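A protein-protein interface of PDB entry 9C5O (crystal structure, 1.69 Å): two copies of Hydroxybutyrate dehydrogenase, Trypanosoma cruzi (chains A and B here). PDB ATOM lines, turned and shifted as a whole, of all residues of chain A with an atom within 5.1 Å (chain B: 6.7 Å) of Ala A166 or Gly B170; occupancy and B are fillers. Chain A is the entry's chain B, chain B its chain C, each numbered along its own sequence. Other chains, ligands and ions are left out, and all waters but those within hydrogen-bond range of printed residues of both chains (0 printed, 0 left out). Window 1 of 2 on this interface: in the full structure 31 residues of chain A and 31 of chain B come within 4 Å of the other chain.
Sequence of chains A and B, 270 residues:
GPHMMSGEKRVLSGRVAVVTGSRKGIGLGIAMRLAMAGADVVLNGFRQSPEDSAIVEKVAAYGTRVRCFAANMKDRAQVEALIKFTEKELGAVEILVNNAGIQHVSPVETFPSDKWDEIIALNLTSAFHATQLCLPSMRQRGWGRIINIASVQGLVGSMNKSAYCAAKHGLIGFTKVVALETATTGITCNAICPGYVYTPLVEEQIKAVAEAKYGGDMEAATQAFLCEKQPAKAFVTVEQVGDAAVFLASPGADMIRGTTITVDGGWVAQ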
ATOM      1  N   TRP A 116      32.604  21.182  -8.146  1.00  0.00           N
ATOM      2  CA  TRP A 116      32.028  20.081  -7.390  1.00  0.00           C
ATOM      3  C   TRP A 116      31.870  20.494  -5.937  1.00  0.00           C
ATOM      4  O   TRP A 116      30.770  20.420  -5.368  1.00  0.00           O
ATOM      5  CB  TRP A 116      32.921  18.840  -7.513  1.00  0.00           C
ATOM      6  CG  TRP A 116      32.493  17.730  -6.594  1.00  0.00           C
ATOM      7  CD1 TRP A 116      32.790  17.608  -5.258  1.00  0.00           C
ATOM      8  CD2 TRP A 116      31.662  16.610  -6.920  1.00  0.00           C
ATOM      9  NE1 TRP A 116      32.206  16.478  -4.742  1.00  0.00           N
ATOM     10  CE2 TRP A 116      31.511  15.841  -5.735  1.00  0.00           C
ATOM     11  CE3 TRP A 116      31.051  16.165  -8.096  1.00  0.00           C
ATOM     12  CZ2 TRP A 116      30.762  14.665  -5.692  1.00  0.00           C
ATOM     13  CZ3 TRP A 116      30.315  14.983  -8.057  1.00  0.00           C
ATOM     14  CH2 TRP A 116      30.153  14.264  -6.846  1.00  0.00           C
ATOM     15  N   ILE A 120      28.311  20.904  -3.730  1.00  0.00           N
ATOM     16  CA  ILE A 120      28.031  20.160  -2.501  1.00  0.00           C
ATOM     17  C   ILE A 120      27.836  21.123  -1.327  1.00  0.00           C
ATOM     18  O   ILE A 120      26.898  20.978  -0.526  1.00  0.00           O
ATOM     19  CB  ILE A 120      29.148  19.151  -2.193  1.00  0.00           C
ATOM     20  CG1 ILE A 120      29.342  18.122  -3.317  1.00  0.00           C
ATOM     21  CG2 ILE A 120      28.876  18.468  -0.842  1.00  0.00           C
ATOM     22  CD1 ILE A 120      28.174  17.308  -3.624  1.00  0.00           C
ATOM     23  N   LYS A 161      25.453  16.221 -14.922  1.00  0.00           N
ATOM     24  CA  LYS A 161      25.036  16.927 -13.728  1.00  0.00           C
ATOM     25  C   LYS A 161      25.388  16.108 -12.499  1.00  0.00           C
ATOM     26  O   LYS A 161      24.628  16.038 -11.524  1.00  0.00           O
ATOM     27  CB  LYS A 161      23.549  17.254 -13.796  1.00  0.00           C
ATOM     28  CG  LYS A 161      23.217  18.227 -14.891  1.00  0.00           C
ATOM     29  CD  LYS A 161      21.702  18.529 -14.980  1.00  0.00           C
ATOM     30  CE  LYS A 161      21.442  19.582 -16.035  1.00  0.00           C
ATOM     31  NZ  LYS A 161      20.012  19.975 -16.129  1.00  0.00           N
ATOM     32  N   SER A 162      26.576  15.496 -12.523  1.00  0.00           N
ATOM     33  CA  SER A 162      26.954  14.597 -11.428  1.00  0.00           C
ATOM     34  C   SER A 162      26.925  15.294 -10.073  1.00  0.00           C
ATOM     35  O   SER A 162      26.375  14.754  -9.102  1.00  0.00           O
ATOM     36  CB  SER A 162      28.340  13.992 -11.683  1.00  0.00           C
ATOM     37  OG  SER A 162      29.388  14.946 -11.874  1.00  0.00           O
ATOM     38  N   ALA A 163      27.547  16.469  -9.959  1.00  0.00           N
ATOM     39  CA  ALA A 163      27.622  17.109  -8.644  1.00  0.00           C
ATOM     40  C   ALA A 163      26.256  17.517  -8.139  1.00  0.00           C
ATOM     41  O   ALA A 163      25.933  17.318  -6.958  1.00  0.00           O
ATOM     42  CB  ALA A 163      28.535  18.339  -8.684  1.00  0.00           C
ATOM     43  N   TYR A 164      25.449  18.107  -9.028  1.00  0.00           N
ATOM     44  CA  TYR A 164      24.097  18.543  -8.696  1.00  0.00           C
ATOM     45  C   TYR A 164      23.201  17.369  -8.310  1.00  0.00           C
ATOM     46  O   TYR A 164      22.475  17.441  -7.317  1.00  0.00           O
ATOM     47  CB  TYR A 164      23.546  19.293  -9.889  1.00  0.00           C
ATOM     48  CG  TYR A 164      22.250  20.033  -9.643  1.00  0.00           C
ATOM     49  CD1 TYR A 164      22.265  21.339  -9.169  1.00  0.00           C
ATOM     50  CD2 TYR A 164      21.035  19.482  -9.987  1.00  0.00           C
ATOM     51  CE1 TYR A 164      21.097  22.054  -9.010  1.00  0.00           C
ATOM     52  CE2 TYR A 164      19.874  20.191  -9.834  1.00  0.00           C
ATOM     53  CZ  TYR A 164      19.913  21.487  -9.337  1.00  0.00           C
ATOM     54  OH  TYR A 164      18.750  22.220  -9.172  1.00  0.00           O
ATOM     55  N   CYS A 165      23.248  16.269  -9.073  1.00  0.00           N
ATOM     56  CA  CYS A 165      22.433  15.117  -8.725  1.00  0.00           C
ATOM     57  C   CYS A 165      22.878  14.537  -7.391  1.00  0.00           C
ATOM     58  O   CYS A 165      22.038  14.145  -6.576  1.00  0.00           O
ATOM     59  CB  CYS A 165      22.476  14.047  -9.818  1.00  0.00           C
ATOM     60  SG  CYS A 165      21.651  14.522 -11.351  1.00  0.00           S
ATOM     61  N   ALA A 166      24.194  14.482  -7.147  1.00  0.00           N
ATOM     62  CA  ALA A 166      24.668  14.000  -5.854  1.00  0.00           C
ATOM     63  C   ALA A 166      24.174  14.895  -4.723  1.00  0.00           C
ATOM     64  O   ALA A 166      23.652  14.410  -3.710  1.00  0.00           O
ATOM     65  CB  ALA A 166      26.187  13.900  -5.860  1.00  0.00           C
ATOM     66  N   ALA A 167      24.299  16.212  -4.886  1.00  0.00           N
ATOM     67  CA  ALA A 167      23.903  17.114  -3.812  1.00  0.00           C
ATOM     68  C   ALA A 167      22.401  17.059  -3.565  1.00  0.00           C
ATOM     69  O   ALA A 167      21.951  17.068  -2.414  1.00  0.00           O
ATOM     70  CB  ALA A 167      24.328  18.538  -4.147  1.00  0.00           C
ATOM     71  N   LYS A 168      21.598  17.036  -4.637  1.00  0.00           N
ATOM     72  CA  LYS A 168      20.143  17.033  -4.476  1.00  0.00           C
ATOM     73  C   LYS A 168      19.612  15.706  -3.923  1.00  0.00           C
ATOM     74  O   LYS A 168      18.712  15.712  -3.066  1.00  0.00           O
ATOM     75  CB  LYS A 168      19.457  17.368  -5.799  1.00  0.00           C
ATOM     76  CG  LYS A 168      19.753  18.820  -6.285  1.00  0.00           C
ATOM     77  CD  LYS A 168      19.329  19.879  -5.252  1.00  0.00           C
ATOM     78  CE  LYS A 168      19.196  21.249  -5.947  1.00  0.00           C
ATOM     79  NZ  LYS A 168      18.636  22.286  -5.072  1.00  0.00           N
ATOM     80  N   HIS A 169      20.150  14.563  -4.382  1.00  0.00           N
ATOM     81  CA  HIS A 169      19.885  13.291  -3.724  1.00  0.00           C
ATOM     82  C   HIS A 169      20.228  13.369  -2.234  1.00  0.00           C
ATOM     83  O   HIS A 169      19.435  12.954  -1.375  1.00  0.00           O
ATOM     84  CB  HIS A 169      20.674  12.153  -4.372  1.00  0.00           C
ATOM     85  CG  HIS A 169      20.023  11.533  -5.579  1.00  0.00           C
ATOM     86  ND1 HIS A 169      19.888  12.194  -6.777  1.00  0.00           N
ATOM     87  CD2 HIS A 169      19.466  10.310  -5.760  1.00  0.00           C
ATOM     88  CE1 HIS A 169      19.315  11.393  -7.662  1.00  0.00           C
ATOM     89  NE2 HIS A 169      19.056  10.237  -7.074  1.00  0.00           N
ATOM     90  N   GLY A 170      21.406  13.924  -1.903  1.00  0.00           N
ATOM     91  CA  GLY A 170      21.793  14.045  -0.505  1.00  0.00           C
ATOM     92  C   GLY A 170      20.832  14.896   0.308  1.00  0.00           C
ATOM     93  O   GLY A 170      20.565  14.602   1.484  1.00  0.00           O
ATOM     94  N   LEU A 171      20.312  15.971  -0.300  1.00  0.00           N
ATOM     95  CA  LEU A 171      19.373  16.847   0.398  1.00  0.00           C
ATOM     96  C   LEU A 171      18.064  16.115   0.713  1.00  0.00           C
ATOM     97  O   LEU A 171      17.460  16.321   1.777  1.00  0.00           O
ATOM     98  CB  LEU A 171      19.098  18.096  -0.456  1.00  0.00           C
ATOM     99  CG  LEU A 171      18.202  19.115   0.227  1.00  0.00           C
ATOM    100  CD1 LEU A 171      18.808  19.662   1.449  1.00  0.00           C
ATOM    101  CD2 LEU A 171      17.973  20.223  -0.822  1.00  0.00           C
ATOM    102  N   LEU B 124      31.198  10.928  -0.923  1.00  0.00           N
ATOM    103  CA  LEU B 124      30.905  11.508  -2.220  1.00  0.00           C
ATOM    104  C   LEU B 124      32.157  11.973  -2.948  1.00  0.00           C
ATOM    105  O   LEU B 124      32.478  11.486  -4.036  1.00  0.00           O
ATOM    106  CB  LEU B 124      29.939  12.681  -2.025  1.00  0.00           C
ATOM    107  CG  LEU B 124      28.520  12.402  -1.604  1.00  0.00           C
ATOM    108  CD1 LEU B 124      27.742  13.720  -1.716  1.00  0.00           C
ATOM    109  CD2 LEU B 124      27.894  11.328  -2.457  1.00  0.00           C
ATOM    110  N   GLY B 154      21.028   5.067   1.910  1.00  0.00           N
ATOM    111  CA  GLY B 154      20.952   5.828   0.677  1.00  0.00           C
ATOM    112  C   GLY B 154      19.588   5.807   0.005  1.00  0.00           C
ATOM    113  O   GLY B 154      19.381   6.525  -0.976  1.00  0.00           O
ATOM    114  N   TYR B 164      25.329  10.501   7.240  1.00  0.00           N
ATOM    115  CA  TYR B 164      25.491   9.242   6.531  1.00  0.00           C
ATOM    116  C   TYR B 164      24.378   9.043   5.505  1.00  0.00           C
ATOM    117  O   TYR B 164      24.644   8.652   4.365  1.00  0.00           O
ATOM    118  CB  TYR B 164      25.526   8.134   7.563  1.00  0.00           C
ATOM    119  CG  TYR B 164      25.895   6.760   7.050  1.00  0.00           C
ATOM    120  CD1 TYR B 164      27.236   6.339   6.987  1.00  0.00           C
ATOM    121  CD2 TYR B 164      24.915   5.855   6.690  1.00  0.00           C
ATOM    122  CE1 TYR B 164      27.555   5.064   6.567  1.00  0.00           C
ATOM    123  CE2 TYR B 164      25.245   4.565   6.289  1.00  0.00           C
ATOM    124  CZ  TYR B 164      26.551   4.185   6.219  1.00  0.00           C
ATOM    125  OH  TYR B 164      26.865   2.903   5.805  1.00  0.00           O
ATOM    126  N   CYS B 165      23.135   9.301   5.886  1.00  0.00           N
ATOM    127  CA  CYS B 165      22.040   9.185   4.932  1.00  0.00           C
ATOM    128  C   CYS B 165      22.187  10.177   3.789  1.00  0.00           C
ATOM    129  O   CYS B 165      21.933   9.833   2.624  1.00  0.00           O
ATOM    130  CB  CYS B 165      20.701   9.382   5.641  1.00  0.00           C
ATOM    131  SG  CYS B 165      20.251   8.052   6.771  1.00  0.00           S
ATOM    132  N   ALA B 166      22.599  11.414   4.083  1.00  0.00           N
ATOM    133  CA  ALA B 166      22.816  12.372   3.004  1.00  0.00           C
ATOM    134  C   ALA B 166      23.930  11.909   2.062  1.00  0.00           C
ATOM    135  O   ALA B 166      23.777  11.937   0.843  1.00  0.00           O
ATOM    136  CB  ALA B 166      23.128  13.735   3.599  1.00  0.00           C
ATOM    137  N   ALA B 167      25.055  11.440   2.619  1.00  0.00           N
ATOM    138  CA  ALA B 167      26.169  10.962   1.802  1.00  0.00           C
ATOM    139  C   ALA B 167      25.787   9.746   0.959  1.00  0.00           C
ATOM    140  O   ALA B 167      26.134   9.665  -0.225  1.00  0.00           O
ATOM    141  CB  ALA B 167      27.337  10.632   2.725  1.00  0.00           C
ATOM    142  N   LYS B 168      25.077   8.792   1.548  1.00  0.00           N
ATOM    143  CA  LYS B 168      24.726   7.574   0.821  1.00  0.00           C
ATOM    144  C   LYS B 168      23.659   7.835  -0.251  1.00  0.00           C
ATOM    145  O   LYS B 168      23.713   7.245  -1.349  1.00  0.00           O
ATOM    146  CB  LYS B 168      24.276   6.511   1.807  1.00  0.00           C
ATOM    147  CG  LYS B 168      25.418   6.013   2.735  1.00  0.00           C
ATOM    148  CD  LYS B 168      26.588   5.452   1.948  1.00  0.00           C
ATOM    149  CE  LYS B 168      27.596   4.719   2.914  1.00  0.00           C
ATOM    150  NZ  LYS B 168      28.781   4.231   2.149  1.00  0.00           N
ATOM    151  N   HIS B 169      22.692   8.715   0.034  1.00  0.00           N
ATOM    152  CA  HIS B 169      21.761   9.144  -1.001  1.00  0.00           C
ATOM    153  C   HIS B 169      22.536   9.822  -2.127  1.00  0.00           C
ATOM    154  O   HIS B 169      22.330   9.527  -3.305  1.00  0.00           O
ATOM    155  CB  HIS B 169      20.712  10.111  -0.439  1.00  0.00           C
ATOM    156  CG  HIS B 169      19.517   9.460   0.191  1.00  0.00           C
ATOM    157  ND1 HIS B 169      19.591   8.788   1.394  1.00  0.00           N
ATOM    158  CD2 HIS B 169      18.217   9.426  -0.185  1.00  0.00           C
ATOM    159  CE1 HIS B 169      18.381   8.369   1.733  1.00  0.00           C
ATOM    160  NE2 HIS B 169      17.533   8.734   0.784  1.00  0.00           N
ATOM    161  N   GLY B 170      23.474  10.717  -1.767  1.00  0.00           N
ATOM    162  CA  GLY B 170      24.267  11.379  -2.783  1.00  0.00           C
ATOM    163  C   GLY B 170      25.042  10.398  -3.650  1.00  0.00           C
ATOM    164  O   GLY B 170      25.179  10.598  -4.857  1.00  0.00           O
ATOM    165  N   LEU B 171      25.605   9.352  -3.029  1.00  0.00           N
ATOM    166  CA  LEU B 171      26.411   8.383  -3.774  1.00  0.00           C
ATOM    167  C   LEU B 171      25.552   7.620  -4.775  1.00  0.00           C
ATOM    168  O   LEU B 171      25.996   7.327  -5.895  1.00  0.00           O
ATOM    169  CB  LEU B 171      27.097   7.421  -2.802  1.00  0.00           C
ATOM    170  CG  LEU B 171      28.036   6.372  -3.404  1.00  0.00           C
ATOM    171  CD1 LEU B 171      29.146   7.090  -4.193  1.00  0.00           C
ATOM    172  CD2 LEU B 171      28.621   5.497  -2.304  1.00  0.00           C
ATOM    173  N   ILE B 172      24.295   7.359  -4.414  1.00  0.00           N
ATOM    174  CA  ILE B 172      23.369   6.735  -5.373  1.00  0.00           C
ATOM    175  C   ILE B 172      23.046   7.694  -6.535  1.00  0.00           C
ATOM    176  O   ILE B 172      22.981   7.285  -7.705  1.00  0.00           O
ATOM    177  CB  ILE B 172      22.102   6.272  -4.626  1.00  0.00           C
ATOM    178  CG1 ILE B 172      22.435   5.012  -3.788  1.00  0.00           C
ATOM    179  CG2 ILE B 172      20.962   5.951  -5.570  1.00  0.00           C
ATOM    180  CD1 ILE B 172      21.432   4.607  -2.753  1.00  0.00           C
ATOM    181  N   GLY B 173      22.839   8.982  -6.235  1.00  0.00           N
ATOM    182  CA  GLY B 173      22.631   9.946  -7.323  1.00  0.00           C
ATOM    183  C   GLY B 173      23.825  10.026  -8.263  1.00  0.00           C
ATOM    184  O   GLY B 173      23.687  10.037  -9.511  1.00  0.00           O
ATOM    185  N   PHE B 174      25.019  10.091  -7.679  1.00  0.00           N
ATOM    186  CA  PHE B 174      26.241  10.086  -8.477  1.00  0.00           C
ATOM    187  C   PHE B 174      26.282   8.856  -9.378  1.00  0.00           C
ATOM    188  O   PHE B 174      26.647   8.950 -10.555  1.00  0.00           O
ATOM    189  CB  PHE B 174      27.456  10.115  -7.536  1.00  0.00           C
ATOM    190  CG  PHE B 174      28.780  10.114  -8.255  1.00  0.00           C
ATOM    191  CD1 PHE B 174      29.167  11.211  -9.015  1.00  0.00           C
ATOM    192  CD2 PHE B 174      29.627   9.048  -8.158  1.00  0.00           C
ATOM    193  CE1 PHE B 174      30.374  11.232  -9.685  1.00  0.00           C
ATOM    194  CE2 PHE B 174      30.870   9.065  -8.841  1.00  0.00           C
ATOM    195  CZ  PHE B 174      31.223  10.154  -9.596  1.00  0.00           C
ATOM    196  N   THR B 175      25.972   7.686  -8.806  1.00  0.00           N
ATOM    197  CA  THR B 175      25.949   6.420  -9.533  1.00  0.00           C
ATOM    198  C   THR B 175      25.085   6.512 -10.777  1.00  0.00           C
ATOM    199  O   THR B 175      25.479   6.058 -11.873  1.00  0.00           O
ATOM    200  CB  THR B 175      25.445   5.304  -8.610  1.00  0.00           C
ATOM    201  OG1 THR B 175      26.344   5.132  -7.502  1.00  0.00           O
ATOM    202  CG2 THR B 175      25.346   3.979  -9.323  1.00  0.00           C
ATOM    203  N   VAL B 177      24.249   9.158 -12.506  1.00  0.00           N
ATOM    204  CA  VAL B 177      24.812  10.038 -13.533  1.00  0.00           C
ATOM    205  C   VAL B 177      25.964   9.350 -14.284  1.00  0.00           C
ATOM    206  O   VAL B 177      26.028   9.372 -15.526  1.00  0.00           O
ATOM    207  CB  VAL B 177      25.251  11.370 -12.909  1.00  0.00           C
ATOM    208  CG1 VAL B 177      26.006  12.204 -13.952  1.00  0.00           C
ATOM    209  CG2 VAL B 177      24.039  12.148 -12.365  1.00  0.00           C
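Tyr A164 touches none of the printed residues of chain B. Of the printed residues of chain B, Ala A166 touches Gly B170. Tyr B164 touches none of the printed residues of chain A. Printed residues of chain A within 4 Å of His B169: His A169. Of the printed residues of chain A, Gly B170 touches Ala A166 and Gly A170. Printed residues of chain A within 4 Å of Val B177: Ser A162 and Cys A165. The nearest residue of chain B that does not touch Ala A166 is Phe B174 (4.3 Å). The nearest printed residue of chain A that does not touch Gly B170 is His A169 (4.004 Å).
Leu B124 touches Trp A116 (O to CZ2, 3.97 Å). Phe B174 touches Trp A116 (CD1 to CH2, 3.9 Å). Ser A162 touches Phe B174 (CB to CD1, 3.9 Å). Val B177 touches Ser A162. Val B177 touches Cys A165 (CG2 to SG, 3.5 Å). Ala A166 touches Gly B170. His A169 touches His B169 (O to CB, 3.3 Å). CG of His A169 touches CA of Gly B173, 3.5 Å away. O of Ala B166 touches CA of Gly A170, at 3.2 Å. N of Gly B170 touches N of Gly A170 (3.8 Å).
Of the 15 printed residues of chain B, 7 touch a printed residue of chain A. Among the printed residues, no Asp or Glu carboxylate lies within 4 Å of a Lys or Arg side-chain nitrogen of the other chain.
Ala A166 touches Gly B170, and with the chains exchanged Gly A170 touches Ala B166. His B169 touches its own counterpart, His A169. Gly B170 touches its own counterpart, Gly A170. 8 positions are printed for both chains. Of the 10 pairs that touch across the chains among the printed residues, 4 have their exchanged pair printed and touching as well.
The backbone carbonyl oxygen of Cys A165 lies within hydrogen-bond range of a ring nitrogen (ND1) of His A169, 2.9 Å away. ND1 of His B169 is in hydrogen-bond range of O of Cys B165. A ring nitrogen (ND1) of His B169 sits close to the backbone carbonyl oxygen (O) of Gly B154 (3.3 Å). The side-chain sulfur (SG) of Cys A165 is in hydrogen-bond range of the backbone carbonyl oxygen (O) of Lys A161 (3.3 Å).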
